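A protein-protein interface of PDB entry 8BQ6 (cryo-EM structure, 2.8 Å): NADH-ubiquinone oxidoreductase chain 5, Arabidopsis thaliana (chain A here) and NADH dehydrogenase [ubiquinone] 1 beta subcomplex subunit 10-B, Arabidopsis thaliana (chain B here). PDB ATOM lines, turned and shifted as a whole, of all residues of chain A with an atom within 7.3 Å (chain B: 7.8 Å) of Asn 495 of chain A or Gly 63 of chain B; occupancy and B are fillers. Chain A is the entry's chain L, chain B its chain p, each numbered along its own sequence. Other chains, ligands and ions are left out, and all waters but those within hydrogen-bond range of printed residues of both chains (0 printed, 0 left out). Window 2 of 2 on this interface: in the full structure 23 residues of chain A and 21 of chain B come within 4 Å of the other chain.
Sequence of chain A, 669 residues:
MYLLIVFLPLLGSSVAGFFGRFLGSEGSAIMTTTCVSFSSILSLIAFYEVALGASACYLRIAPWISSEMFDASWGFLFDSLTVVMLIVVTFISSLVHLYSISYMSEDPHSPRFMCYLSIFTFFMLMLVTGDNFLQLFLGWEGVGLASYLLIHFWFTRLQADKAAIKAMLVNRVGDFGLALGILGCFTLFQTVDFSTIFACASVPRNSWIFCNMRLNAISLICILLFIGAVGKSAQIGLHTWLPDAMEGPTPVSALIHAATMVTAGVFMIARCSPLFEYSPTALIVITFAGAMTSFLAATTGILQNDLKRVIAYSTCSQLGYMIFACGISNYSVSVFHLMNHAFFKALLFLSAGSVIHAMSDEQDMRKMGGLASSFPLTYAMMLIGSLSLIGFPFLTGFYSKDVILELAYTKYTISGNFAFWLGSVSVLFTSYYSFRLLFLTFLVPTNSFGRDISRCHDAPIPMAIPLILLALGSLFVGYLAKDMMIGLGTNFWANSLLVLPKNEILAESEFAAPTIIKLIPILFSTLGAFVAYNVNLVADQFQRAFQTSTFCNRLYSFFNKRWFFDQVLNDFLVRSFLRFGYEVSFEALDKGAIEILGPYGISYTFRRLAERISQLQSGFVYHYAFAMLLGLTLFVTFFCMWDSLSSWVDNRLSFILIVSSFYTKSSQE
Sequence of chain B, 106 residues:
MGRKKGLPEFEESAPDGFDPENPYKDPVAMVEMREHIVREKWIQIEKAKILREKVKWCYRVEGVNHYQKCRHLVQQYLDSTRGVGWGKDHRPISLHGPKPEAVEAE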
ATOM      1  N   TYR A  58      35.315  -5.108  -4.935  1.00  0.00           N
ATOM      2  CA  TYR A  58      35.234  -6.174  -5.922  1.00  0.00           C
ATOM      3  C   TYR A  58      36.564  -6.269  -6.644  1.00  0.00           C
ATOM      4  O   TYR A  58      37.101  -5.256  -7.100  1.00  0.00           O
ATOM      5  CB  TYR A  58      34.097  -5.927  -6.911  1.00  0.00           C
ATOM      6  CG  TYR A  58      32.781  -5.771  -6.213  1.00  0.00           C
ATOM      7  CD1 TYR A  58      32.038  -6.883  -5.863  1.00  0.00           C
ATOM      8  CD2 TYR A  58      32.294  -4.518  -5.872  1.00  0.00           C
ATOM      9  CE1 TYR A  58      30.845  -6.761  -5.208  1.00  0.00           C
ATOM     10  CE2 TYR A  58      31.090  -4.385  -5.213  1.00  0.00           C
ATOM     11  CZ  TYR A  58      30.371  -5.514  -4.885  1.00  0.00           C
ATOM     12  OH  TYR A  58      29.168  -5.413  -4.231  1.00  0.00           O
ATOM     13  N   ASP A  79      32.115  -7.826   0.970  1.00  0.00           N
ATOM     14  CA  ASP A  79      30.972  -7.080   1.466  1.00  0.00           C
ATOM     15  C   ASP A  79      30.900  -7.257   2.980  1.00  0.00           C
ATOM     16  O   ASP A  79      31.829  -7.769   3.610  1.00  0.00           O
ATOM     17  CB  ASP A  79      29.676  -7.504   0.771  1.00  0.00           C
ATOM     18  CG  ASP A  79      29.307  -8.947   1.029  1.00  0.00           C
ATOM     19  OD1 ASP A  79      30.051  -9.666   1.727  1.00  0.00           O
ATOM     20  OD2 ASP A  79      28.233  -9.357   0.548  1.00  0.00           O
ATOM     21  N   SER A  80      29.779  -6.824   3.557  1.00  0.00           N
ATOM     22  CA  SER A  80      29.646  -6.800   5.008  1.00  0.00           C
ATOM     23  C   SER A  80      29.745  -8.199   5.605  1.00  0.00           C
ATOM     24  O   SER A  80      30.365  -8.393   6.656  1.00  0.00           O
ATOM     25  CB  SER A  80      28.324  -6.139   5.388  1.00  0.00           C
ATOM     26  OG  SER A  80      28.435  -4.735   5.265  1.00  0.00           O
ATOM     27  N   PHE A 198      22.116 -13.883  -7.714  1.00  0.00           N
ATOM     28  CA  PHE A 198      21.258 -13.240  -6.728  1.00  0.00           C
ATOM     29  C   PHE A 198      20.349 -12.205  -7.376  1.00  0.00           C
ATOM     30  O   PHE A 198      19.207 -12.024  -6.939  1.00  0.00           O
ATOM     31  CB  PHE A 198      22.102 -12.612  -5.619  1.00  0.00           C
ATOM     32  CG  PHE A 198      22.940 -13.606  -4.864  1.00  0.00           C
ATOM     33  CD1 PHE A 198      22.614 -14.952  -4.868  1.00  0.00           C
ATOM     34  CD2 PHE A 198      24.026 -13.191  -4.118  1.00  0.00           C
ATOM     35  CE1 PHE A 198      23.375 -15.867  -4.173  1.00  0.00           C
ATOM     36  CE2 PHE A 198      24.783 -14.102  -3.415  1.00  0.00           C
ATOM     37  CZ  PHE A 198      24.456 -15.443  -3.445  1.00  0.00           C
ATOM     38  N   ARG A 271      25.374 -16.446   2.887  1.00  0.00           N
ATOM     39  CA  ARG A 271      25.837 -15.787   1.670  1.00  0.00           C
ATOM     40  C   ARG A 271      24.866 -15.994   0.516  1.00  0.00           C
ATOM     41  O   ARG A 271      24.718 -15.109  -0.334  1.00  0.00           O
ATOM     42  CB  ARG A 271      27.239 -16.297   1.313  1.00  0.00           C
ATOM     43  CG  ARG A 271      27.594 -16.342  -0.174  1.00  0.00           C
ATOM     44  CD  ARG A 271      28.004 -14.982  -0.717  1.00  0.00           C
ATOM     45  NE  ARG A 271      29.070 -14.371   0.067  1.00  0.00           N
ATOM     46  CZ  ARG A 271      29.135 -13.078   0.354  1.00  0.00           C
ATOM     47  NH1 ARG A 271      28.218 -12.228  -0.078  1.00  0.00           N
ATOM     48  NH2 ARG A 271      30.140 -12.627   1.098  1.00  0.00           N
ATOM     49  N   SER A 273      21.562 -16.358   0.870  1.00  0.00           N
ATOM     50  CA  SER A 273      20.203 -15.998   1.271  1.00  0.00           C
ATOM     51  C   SER A 273      19.348 -15.423   0.141  1.00  0.00           C
ATOM     52  O   SER A 273      18.153 -15.756   0.094  1.00  0.00           O
ATOM     53  CB  SER A 273      20.260 -15.046   2.475  1.00  0.00           C
ATOM     54  OG  SER A 273      21.064 -13.912   2.227  1.00  0.00           O
ATOM     55  N   PRO A 274      19.855 -14.590  -0.780  1.00  0.00           N
ATOM     56  CA  PRO A 274      19.007 -14.171  -1.912  1.00  0.00           C
ATOM     57  C   PRO A 274      18.546 -15.315  -2.800  1.00  0.00           C
ATOM     58  O   PRO A 274      17.620 -15.122  -3.597  1.00  0.00           O
ATOM     59  CB  PRO A 274      19.901 -13.196  -2.690  1.00  0.00           C
ATOM     60  CG  PRO A 274      20.935 -12.775  -1.748  1.00  0.00           C
ATOM     61  CD  PRO A 274      21.163 -13.912  -0.818  1.00  0.00           C
ATOM     62  N   ASN A 491      21.071  -1.263   8.869  1.00  0.00           N
ATOM     63  CA  ASN A 491      21.567  -1.295   7.500  1.00  0.00           C
ATOM     64  C   ASN A 491      23.012  -1.771   7.418  1.00  0.00           C
ATOM     65  O   ASN A 491      23.685  -1.527   6.410  1.00  0.00           O
ATOM     66  CB  ASN A 491      21.454   0.085   6.857  1.00  0.00           C
ATOM     67  CG  ASN A 491      22.270   1.131   7.581  1.00  0.00           C
ATOM     68  OD1 ASN A 491      22.755   0.907   8.692  1.00  0.00           O
ATOM     69  ND2 ASN A 491      22.464   2.271   6.936  1.00  0.00           N
ATOM     70  N   PHE A 492      23.505  -2.421   8.470  1.00  0.00           N
ATOM     71  CA  PHE A 492      24.904  -2.829   8.525  1.00  0.00           C
ATOM     72  C   PHE A 492      25.239  -3.820   7.420  1.00  0.00           C
ATOM     73  O   PHE A 492      26.324  -3.768   6.832  1.00  0.00           O
ATOM     74  CB  PHE A 492      25.187  -3.421   9.902  1.00  0.00           C
ATOM     75  CG  PHE A 492      26.502  -4.123  10.018  1.00  0.00           C
ATOM     76  CD1 PHE A 492      27.682  -3.411  10.084  1.00  0.00           C
ATOM     77  CD2 PHE A 492      26.551  -5.504  10.098  1.00  0.00           C
ATOM     78  CE1 PHE A 492      28.885  -4.063  10.211  1.00  0.00           C
ATOM     79  CE2 PHE A 492      27.754  -6.159  10.221  1.00  0.00           C
ATOM     80  CZ  PHE A 492      28.921  -5.439  10.278  1.00  0.00           C
ATOM     81  N   TRP A 493      24.311  -4.727   7.121  1.00  0.00           N
ATOM     82  CA  TRP A 493      24.551  -5.762   6.129  1.00  0.00           C
ATOM     83  C   TRP A 493      24.382  -5.269   4.702  1.00  0.00           C
ATOM     84  O   TRP A 493      24.789  -5.973   3.773  1.00  0.00           O
ATOM     85  CB  TRP A 493      23.608  -6.934   6.375  1.00  0.00           C
ATOM     86  CG  TRP A 493      23.777  -7.522   7.723  1.00  0.00           C
ATOM     87  CD1 TRP A 493      22.978  -7.329   8.806  1.00  0.00           C
ATOM     88  CD2 TRP A 493      24.823  -8.399   8.143  1.00  0.00           C
ATOM     89  NE1 TRP A 493      23.457  -8.038   9.878  1.00  0.00           N
ATOM     90  CE2 TRP A 493      24.590  -8.705   9.493  1.00  0.00           C
ATOM     91  CE3 TRP A 493      25.930  -8.961   7.504  1.00  0.00           C
ATOM     92  CZ2 TRP A 493      25.420  -9.549  10.215  1.00  0.00           C
ATOM     93  CZ3 TRP A 493      26.756  -9.790   8.224  1.00  0.00           C
ATOM     94  CH2 TRP A 493      26.500 -10.074   9.567  1.00  0.00           C
ATOM     95  N   ALA A 494      23.794  -4.086   4.513  1.00  0.00           N
ATOM     96  CA  ALA A 494      23.563  -3.529   3.185  1.00  0.00           C
ATOM     97  C   ALA A 494      22.811  -4.526   2.314  1.00  0.00           C
ATOM     98  O   ALA A 494      21.644  -4.828   2.577  1.00  0.00           O
ATOM     99  CB  ALA A 494      24.886  -3.127   2.529  1.00  0.00           C
ATOM    100  N   ASN A 495      23.472  -5.053   1.286  1.00  0.00           N
ATOM    101  CA  ASN A 495      22.878  -6.052   0.411  1.00  0.00           C
ATOM    102  C   ASN A 495      23.480  -7.438   0.607  1.00  0.00           C
ATOM    103  O   ASN A 495      23.306  -8.306  -0.255  1.00  0.00           O
ATOM    104  CB  ASN A 495      23.023  -5.627  -1.050  1.00  0.00           C
ATOM    105  CG  ASN A 495      21.904  -6.157  -1.919  1.00  0.00           C
ATOM    106  OD1 ASN A 495      20.850  -6.548  -1.422  1.00  0.00           O
ATOM    107  ND2 ASN A 495      22.135  -6.193  -3.224  1.00  0.00           N
ATOM    108  N   SER A 496      24.191  -7.661   1.713  1.00  0.00           N
ATOM    109  CA  SER A 496      24.841  -8.948   1.938  1.00  0.00           C
ATOM    110  C   SER A 496      23.824 -10.041   2.233  1.00  0.00           C
ATOM    111  O   SER A 496      23.928 -11.156   1.708  1.00  0.00           O
ATOM    112  CB  SER A 496      25.842  -8.829   3.083  1.00  0.00           C
ATOM    113  OG  SER A 496      26.689  -7.713   2.886  1.00  0.00           O
ATOM    114  N   LEU A 497      22.837  -9.744   3.068  1.00  0.00           N
ATOM    115  CA  LEU A 497      21.810 -10.702   3.431  1.00  0.00           C
ATOM    116  C   LEU A 497      20.461 -10.209   2.941  1.00  0.00           C
ATOM    117  O   LEU A 497      20.227  -9.003   2.816  1.00  0.00           O
ATOM    118  CB  LEU A 497      21.769 -10.936   4.943  1.00  0.00           C
ATOM    119  CG  LEU A 497      23.113 -11.377   5.513  1.00  0.00           C
ATOM    120  CD1 LEU A 497      23.161 -11.223   7.021  1.00  0.00           C
ATOM    121  CD2 LEU A 497      23.398 -12.810   5.100  1.00  0.00           C
ATOM    122  N   LEU A 498      19.580 -11.159   2.640  1.00  0.00           N
ATOM    123  CA  LEU A 498      18.249 -10.851   2.143  1.00  0.00           C
ATOM    124  C   LEU A 498      17.215 -11.567   2.993  1.00  0.00           C
ATOM    125  O   LEU A 498      17.278 -12.789   3.157  1.00  0.00           O
ATOM    126  CB  LEU A 498      18.089 -11.249   0.677  1.00  0.00           C
ATOM    127  CG  LEU A 498      16.650 -11.035   0.214  1.00  0.00           C
ATOM    128  CD1 LEU A 498      16.461  -9.609  -0.267  1.00  0.00           C
ATOM    129  CD2 LEU A 498      16.268 -12.022  -0.865  1.00  0.00           C
ATOM    130  N   TRP B  57      26.967  -5.633 -12.493  1.00  0.00           N
ATOM    131  CA  TRP B  57      27.350  -4.349 -11.920  1.00  0.00           C
ATOM    132  C   TRP B  57      26.134  -3.558 -11.451  1.00  0.00           C
ATOM    133  O   TRP B  57      26.258  -2.704 -10.571  1.00  0.00           O
ATOM    134  CB  TRP B  57      28.191  -3.563 -12.923  1.00  0.00           C
ATOM    135  CG  TRP B  57      29.592  -4.083 -12.976  1.00  0.00           C
ATOM    136  CD1 TRP B  57      30.188  -4.719 -14.020  1.00  0.00           C
ATOM    137  CD2 TRP B  57      30.570  -4.031 -11.929  1.00  0.00           C
ATOM    138  NE1 TRP B  57      31.476  -5.061 -13.695  1.00  0.00           N
ATOM    139  CE2 TRP B  57      31.735  -4.649 -12.415  1.00  0.00           C
ATOM    140  CE3 TRP B  57      30.573  -3.514 -10.630  1.00  0.00           C
ATOM    141  CZ2 TRP B  57      32.892  -4.768 -11.650  1.00  0.00           C
ATOM    142  CZ3 TRP B  57      31.723  -3.633  -9.872  1.00  0.00           C
ATOM    143  CH2 TRP B  57      32.865  -4.255 -10.384  1.00  0.00           C
ATOM    144  N   CYS B  58      24.965  -3.841 -12.017  1.00  0.00           N
ATOM    145  CA  CYS B  58      23.733  -3.205 -11.486  1.00  0.00           C
ATOM    146  C   CYS B  58      23.498  -3.717 -10.058  1.00  0.00           C
ATOM    147  O   CYS B  58      23.237  -2.884  -9.192  1.00  0.00           O
ATOM    148  CB  CYS B  58      22.542  -3.523 -12.377  1.00  0.00           C
ATOM    149  SG  CYS B  58      21.074  -2.528 -12.013  1.00  0.00           S
ATOM    150  N   TYR B  59      23.591  -5.030  -9.817  1.00  0.00           N
ATOM    151  CA  TYR B  59      23.448  -5.576  -8.471  1.00  0.00           C
ATOM    152  C   TYR B  59      24.478  -4.961  -7.536  1.00  0.00           C
ATOM    153  O   TYR B  59      24.178  -4.608  -6.391  1.00  0.00           O
ATOM    154  CB  TYR B  59      23.602  -7.101  -8.509  1.00  0.00           C
ATOM    155  CG  TYR B  59      23.304  -7.819  -7.204  1.00  0.00           C
ATOM    156  CD1 TYR B  59      22.032  -8.286  -6.916  1.00  0.00           C
ATOM    157  CD2 TYR B  59      24.303  -8.029  -6.264  1.00  0.00           C
ATOM    158  CE1 TYR B  59      21.764  -8.946  -5.732  1.00  0.00           C
ATOM    159  CE2 TYR B  59      24.043  -8.684  -5.079  1.00  0.00           C
ATOM    160  CZ  TYR B  59      22.773  -9.138  -4.817  1.00  0.00           C
ATOM    161  OH  TYR B  59      22.517  -9.790  -3.634  1.00  0.00           O
ATOM    162  N   ARG B  60      25.712  -4.826  -8.020  1.00  0.00           N
ATOM    163  CA  ARG B  60      26.780  -4.309  -7.177  1.00  0.00           C
ATOM    164  C   ARG B  60      26.598  -2.824  -6.902  1.00  0.00           C
ATOM    165  O   ARG B  60      26.884  -2.350  -5.797  1.00  0.00           O
ATOM    166  CB  ARG B  60      28.129  -4.592  -7.830  1.00  0.00           C
ATOM    167  CG  ARG B  60      28.363  -6.074  -8.014  1.00  0.00           C
ATOM    168  CD  ARG B  60      29.633  -6.373  -8.760  1.00  0.00           C
ATOM    169  NE  ARG B  60      30.031  -7.756  -8.537  1.00  0.00           N
ATOM    170  CZ  ARG B  60      31.195  -8.269  -8.903  1.00  0.00           C
ATOM    171  NH1 ARG B  60      32.100  -7.546  -9.541  1.00  0.00           N
ATOM    172  NH2 ARG B  60      31.460  -9.540  -8.617  1.00  0.00           N
ATOM    173  N   VAL B  61      26.092  -2.079  -7.884  1.00  0.00           N
ATOM    174  CA  VAL B  61      25.973  -0.630  -7.753  1.00  0.00           C
ATOM    175  C   VAL B  61      24.715  -0.244  -6.984  1.00  0.00           C
ATOM    176  O   VAL B  61      24.730   0.701  -6.188  1.00  0.00           O
ATOM    177  CB  VAL B  61      26.014   0.020  -9.147  1.00  0.00           C
ATOM    178  CG1 VAL B  61      25.373   1.396  -9.128  1.00  0.00           C
ATOM    179  CG2 VAL B  61      27.444   0.103  -9.628  1.00  0.00           C
ATOM    180  N   GLU B  62      23.603  -0.944  -7.237  1.00  0.00           N
ATOM    181  CA  GLU B  62      22.288  -0.541  -6.660  1.00  0.00           C
ATOM    182  C   GLU B  62      21.957  -1.216  -5.324  1.00  0.00           C
ATOM    183  O   GLU B  62      21.094  -0.665  -4.620  1.00  0.00           O
ATOM    184  CB  GLU B  62      21.181  -0.769  -7.688  1.00  0.00           C
ATOM    185  CG  GLU B  62      21.461  -0.106  -9.027  1.00  0.00           C
ATOM    186  CD  GLU B  62      21.272   1.400  -9.124  1.00  0.00           C
ATOM    187  OE1 GLU B  62      21.765   2.133  -8.245  1.00  0.00           O
ATOM    188  OE2 GLU B  62      20.651   1.842 -10.101  1.00  0.00           O
ATOM    189  N   GLY B  63      22.564  -2.353  -4.985  1.00  0.00           N
ATOM    190  CA  GLY B  63      22.340  -2.926  -3.670  1.00  0.00           C
ATOM    191  C   GLY B  63      20.893  -3.324  -3.461  1.00  0.00           C
ATOM    192  O   GLY B  63      20.284  -4.006  -4.290  1.00  0.00           O
ATOM    193  N   VAL B  64      20.327  -2.880  -2.334  1.00  0.00           N
ATOM    194  CA  VAL B  64      18.972  -3.264  -1.945  1.00  0.00           C
ATOM    195  C   VAL B  64      17.950  -2.866  -3.004  1.00  0.00           C
ATOM    196  O   VAL B  64      16.889  -3.490  -3.113  1.00  0.00           O
ATOM    197  CB  VAL B  64      18.645  -2.652  -0.561  1.00  0.00           C
ATOM    198  CG1 VAL B  64      17.148  -2.508  -0.349  1.00  0.00           C
ATOM    199  CG2 VAL B  64      19.260  -3.483   0.554  1.00  0.00           C
ATOM    200  N   ASN B  65      18.311  -1.925  -3.890  1.00  0.00           N
ATOM    201  CA  ASN B  65      17.362  -1.426  -4.926  1.00  0.00           C
ATOM    202  C   ASN B  65      17.539  -2.144  -6.268  1.00  0.00           C
ATOM    203  O   ASN B  65      17.054  -1.608  -7.271  1.00  0.00           O
ATOM    204  CB  ASN B  65      17.495   0.086  -5.132  1.00  0.00           C
ATOM    205  CG  ASN B  65      17.576   0.862  -3.834  1.00  0.00           C
ATOM    206  OD1 ASN B  65      16.832   0.590  -2.896  1.00  0.00           O
ATOM    207  ND2 ASN B  65      18.476   1.828  -3.769  1.00  0.00           N
ATOM    208  N   HIS B  66      18.152  -3.331  -6.287  1.00  0.00           N
ATOM    209  CA  HIS B  66      18.445  -4.016  -7.573  1.00  0.00           C
ATOM    210  C   HIS B  66      17.173  -4.581  -8.206  1.00  0.00           C
ATOM    211  O   HIS B  66      17.151  -4.690  -9.434  1.00  0.00           O
ATOM    212  CB  HIS B  66      19.523  -5.096  -7.381  1.00  0.00           C
ATOM    213  CG  HIS B  66      19.049  -6.334  -6.700  1.00  0.00           C
ATOM    214  ND1 HIS B  66      18.646  -7.449  -7.402  1.00  0.00           N
ATOM    215  CD2 HIS B  66      18.927  -6.645  -5.392  1.00  0.00           C
ATOM    216  CE1 HIS B  66      18.294  -8.392  -6.556  1.00  0.00           C
ATOM    217  NE2 HIS B  66      18.458  -7.925  -5.319  1.00  0.00           N
ATOM    218  N   TYR B  67      16.158  -4.919  -7.408  1.00  0.00           N
ATOM    219  CA  TYR B  67      14.937  -5.577  -7.947  1.00  0.00           C
ATOM    220  C   TYR B  67      14.181  -4.610  -8.857  1.00  0.00           C
ATOM    221  O   TYR B  67      13.679  -5.051  -9.906  1.00  0.00           O
ATOM    222  CB  TYR B  67      14.062  -6.074  -6.799  1.00  0.00           C
ATOM    223  CG  TYR B  67      14.521  -7.371  -6.185  1.00  0.00           C
ATOM    224  CD1 TYR B  67      14.829  -7.452  -4.839  1.00  0.00           C
ATOM    225  CD2 TYR B  67      14.656  -8.513  -6.955  1.00  0.00           C
ATOM    226  CE1 TYR B  67      15.255  -8.639  -4.269  1.00  0.00           C
ATOM    227  CE2 TYR B  67      15.082  -9.708  -6.401  1.00  0.00           C
ATOM    228  CZ  TYR B  67      15.387  -9.771  -5.054  1.00  0.00           C
ATOM    229  OH  TYR B  67      15.813 -10.943  -4.501  1.00  0.00           O
ATOM    230  N   GLN B  68      14.114  -3.339  -8.468  1.00  0.00           N
ATOM    231  CA  GLN B  68      13.408  -2.313  -9.269  1.00  0.00           C
ATOM    232  C   GLN B  68      14.357  -1.741 -10.321  1.00  0.00           C
ATOM    233  O   GLN B  68      13.939  -1.655 -11.489  1.00  0.00           O
ATOM    234  CB  GLN B  68      12.933  -1.208  -8.328  1.00  0.00           C
ATOM    235  CG  GLN B  68      12.064  -0.156  -8.999  1.00  0.00           C
ATOM    236  CD  GLN B  68      11.478   0.822  -8.010  1.00  0.00           C
ATOM    237  OE1 GLN B  68      11.636   0.676  -6.800  1.00  0.00           O
ATOM    238  NE2 GLN B  68      10.795   1.833  -8.521  1.00  0.00           N
ATOM    239  N   LYS B  69      15.595  -1.408  -9.941  1.00  0.00           N
ATOM    240  CA  LYS B  69      16.535  -0.735 -10.888  1.00  0.00           C
ATOM    241  C   LYS B  69      17.042  -1.657 -12.008  1.00  0.00           C
ATOM    242  O   LYS B  69      17.403  -1.119 -13.071  1.00  0.00           O
ATOM    243  CB  LYS B  69      17.725  -0.146 -10.124  1.00  0.00           C
ATOM    244  CG  LYS B  69      17.405   1.093  -9.299  1.00  0.00           C
ATOM    245  CD  LYS B  69      16.641   2.143 -10.075  1.00  0.00           C
ATOM    246  CE  LYS B  69      17.529   3.209 -10.680  1.00  0.00           C
ATOM    247  NZ  LYS B  69      18.244   3.988  -9.641  1.00  0.00           N
ATOM    248  N   CYS B  70      17.123  -2.971 -11.792  1.00  0.00           N
ATOM    249  CA  CYS B  70      17.710  -3.836 -12.852  1.00  0.00           C
ATOM    250  C   CYS B  70      16.654  -4.783 -13.430  1.00  0.00           C
ATOM    251  O   CYS B  70      17.043  -5.636 -14.237  1.00  0.00           O
ATOM    252  CB  CYS B  70      18.911  -4.625 -12.344  1.00  0.00           C
ATOM    253  SG  CYS B  70      19.851  -3.800 -11.033  1.00  0.00           S
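Tyr 58 of chain A touches Arg 60 of chain B (CD1 to CZ, 3.4 Å).
CB of Phe 198 of chain A touches OH of Tyr 59 of chain B (3.5 Å).
Phe 198 of chain A touches His 66 of chain B.
Pro 274 of chain A touches Tyr 59 of chain B (CG to OH, 3.9 Å).
O of Ala 494 of chain A touches CG2 of Val 64 of chain B, 3.4 Å away.
CZ of Tyr 59 of chain B touches ND2 of Asn 495 of chain A, at 3.4 Å.
Asn 495 of chain A touches Val 64 of chain B.
CD2 of His 66 of chain B touches ND2 of Asn 495 of chain A, at 3.9 Å.
CD2 of Leu 498 of chain A touches OH of Tyr 67 of chain B (3.8 Å).
OG of Ser 273 of chain A sits at hydrogen-bond distance from N of Leu 498 of chain A (3.2 Å).
SG of Cys 58 of chain B is disulfide-bonded to SG of Cys 70 of chain B, at 2.0 Å.
Of the 14 printed residues of chain B, 6 touch a printed residue of chain A.
Printed residues of chain B that touch a printed residue of chain A: Tyr 59, Arg 60, Gly 63, Val 64, His 66 and Tyr 67.
Along chain B the printed residues that touch a printed residue of chain A span positions 59 to 67.
Printed residues of chain A that touch a printed residue of chain B: Tyr 58, Phe 198, Pro 274, Ala 494, Asn 495 and Leu 498.
Among the printed residues, 10 pairs touch across the chains.
Among the printed residues, no Asp or Glu carboxylate lies within 4 Å of a Lys or Arg side-chain nitrogen of the other chain.
O of Gly 63 of chain B lies within hydrogen-bond range of ND2 of Asn 495 of chain A.
Ala 494 of chain A touches one residue of chain B.
Asn 495 of chain A touches just these residues of chain B: Tyr 59, Gly 63, Val 64 and His 66.
Printed residues of chain A within 4 Å of Tyr 59 of chain B: Phe 198 (3.5 Å), Pro 274 (3.9 Å) and Asn 495 (3.4 Å).
Gly 63 of chain B touches one residue of chain A.
Printed residues of chain A within 4 Å of Val 64 of chain B: Ala 494 (3.4 Å) and Asn 495 (3.7 Å).
Printed residues of chain A within 4 Å of Tyr 67 of chain B: Leu 498 (3.8 Å).
The nearest residue of chain B that does not touch Asn 495 of chain A is Glu 62 of chain B (5.4 Å).
The nearest printed residue of chain B that does not touch Pro 274 of chain A is Tyr 67 of chain B (4.6 Å).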
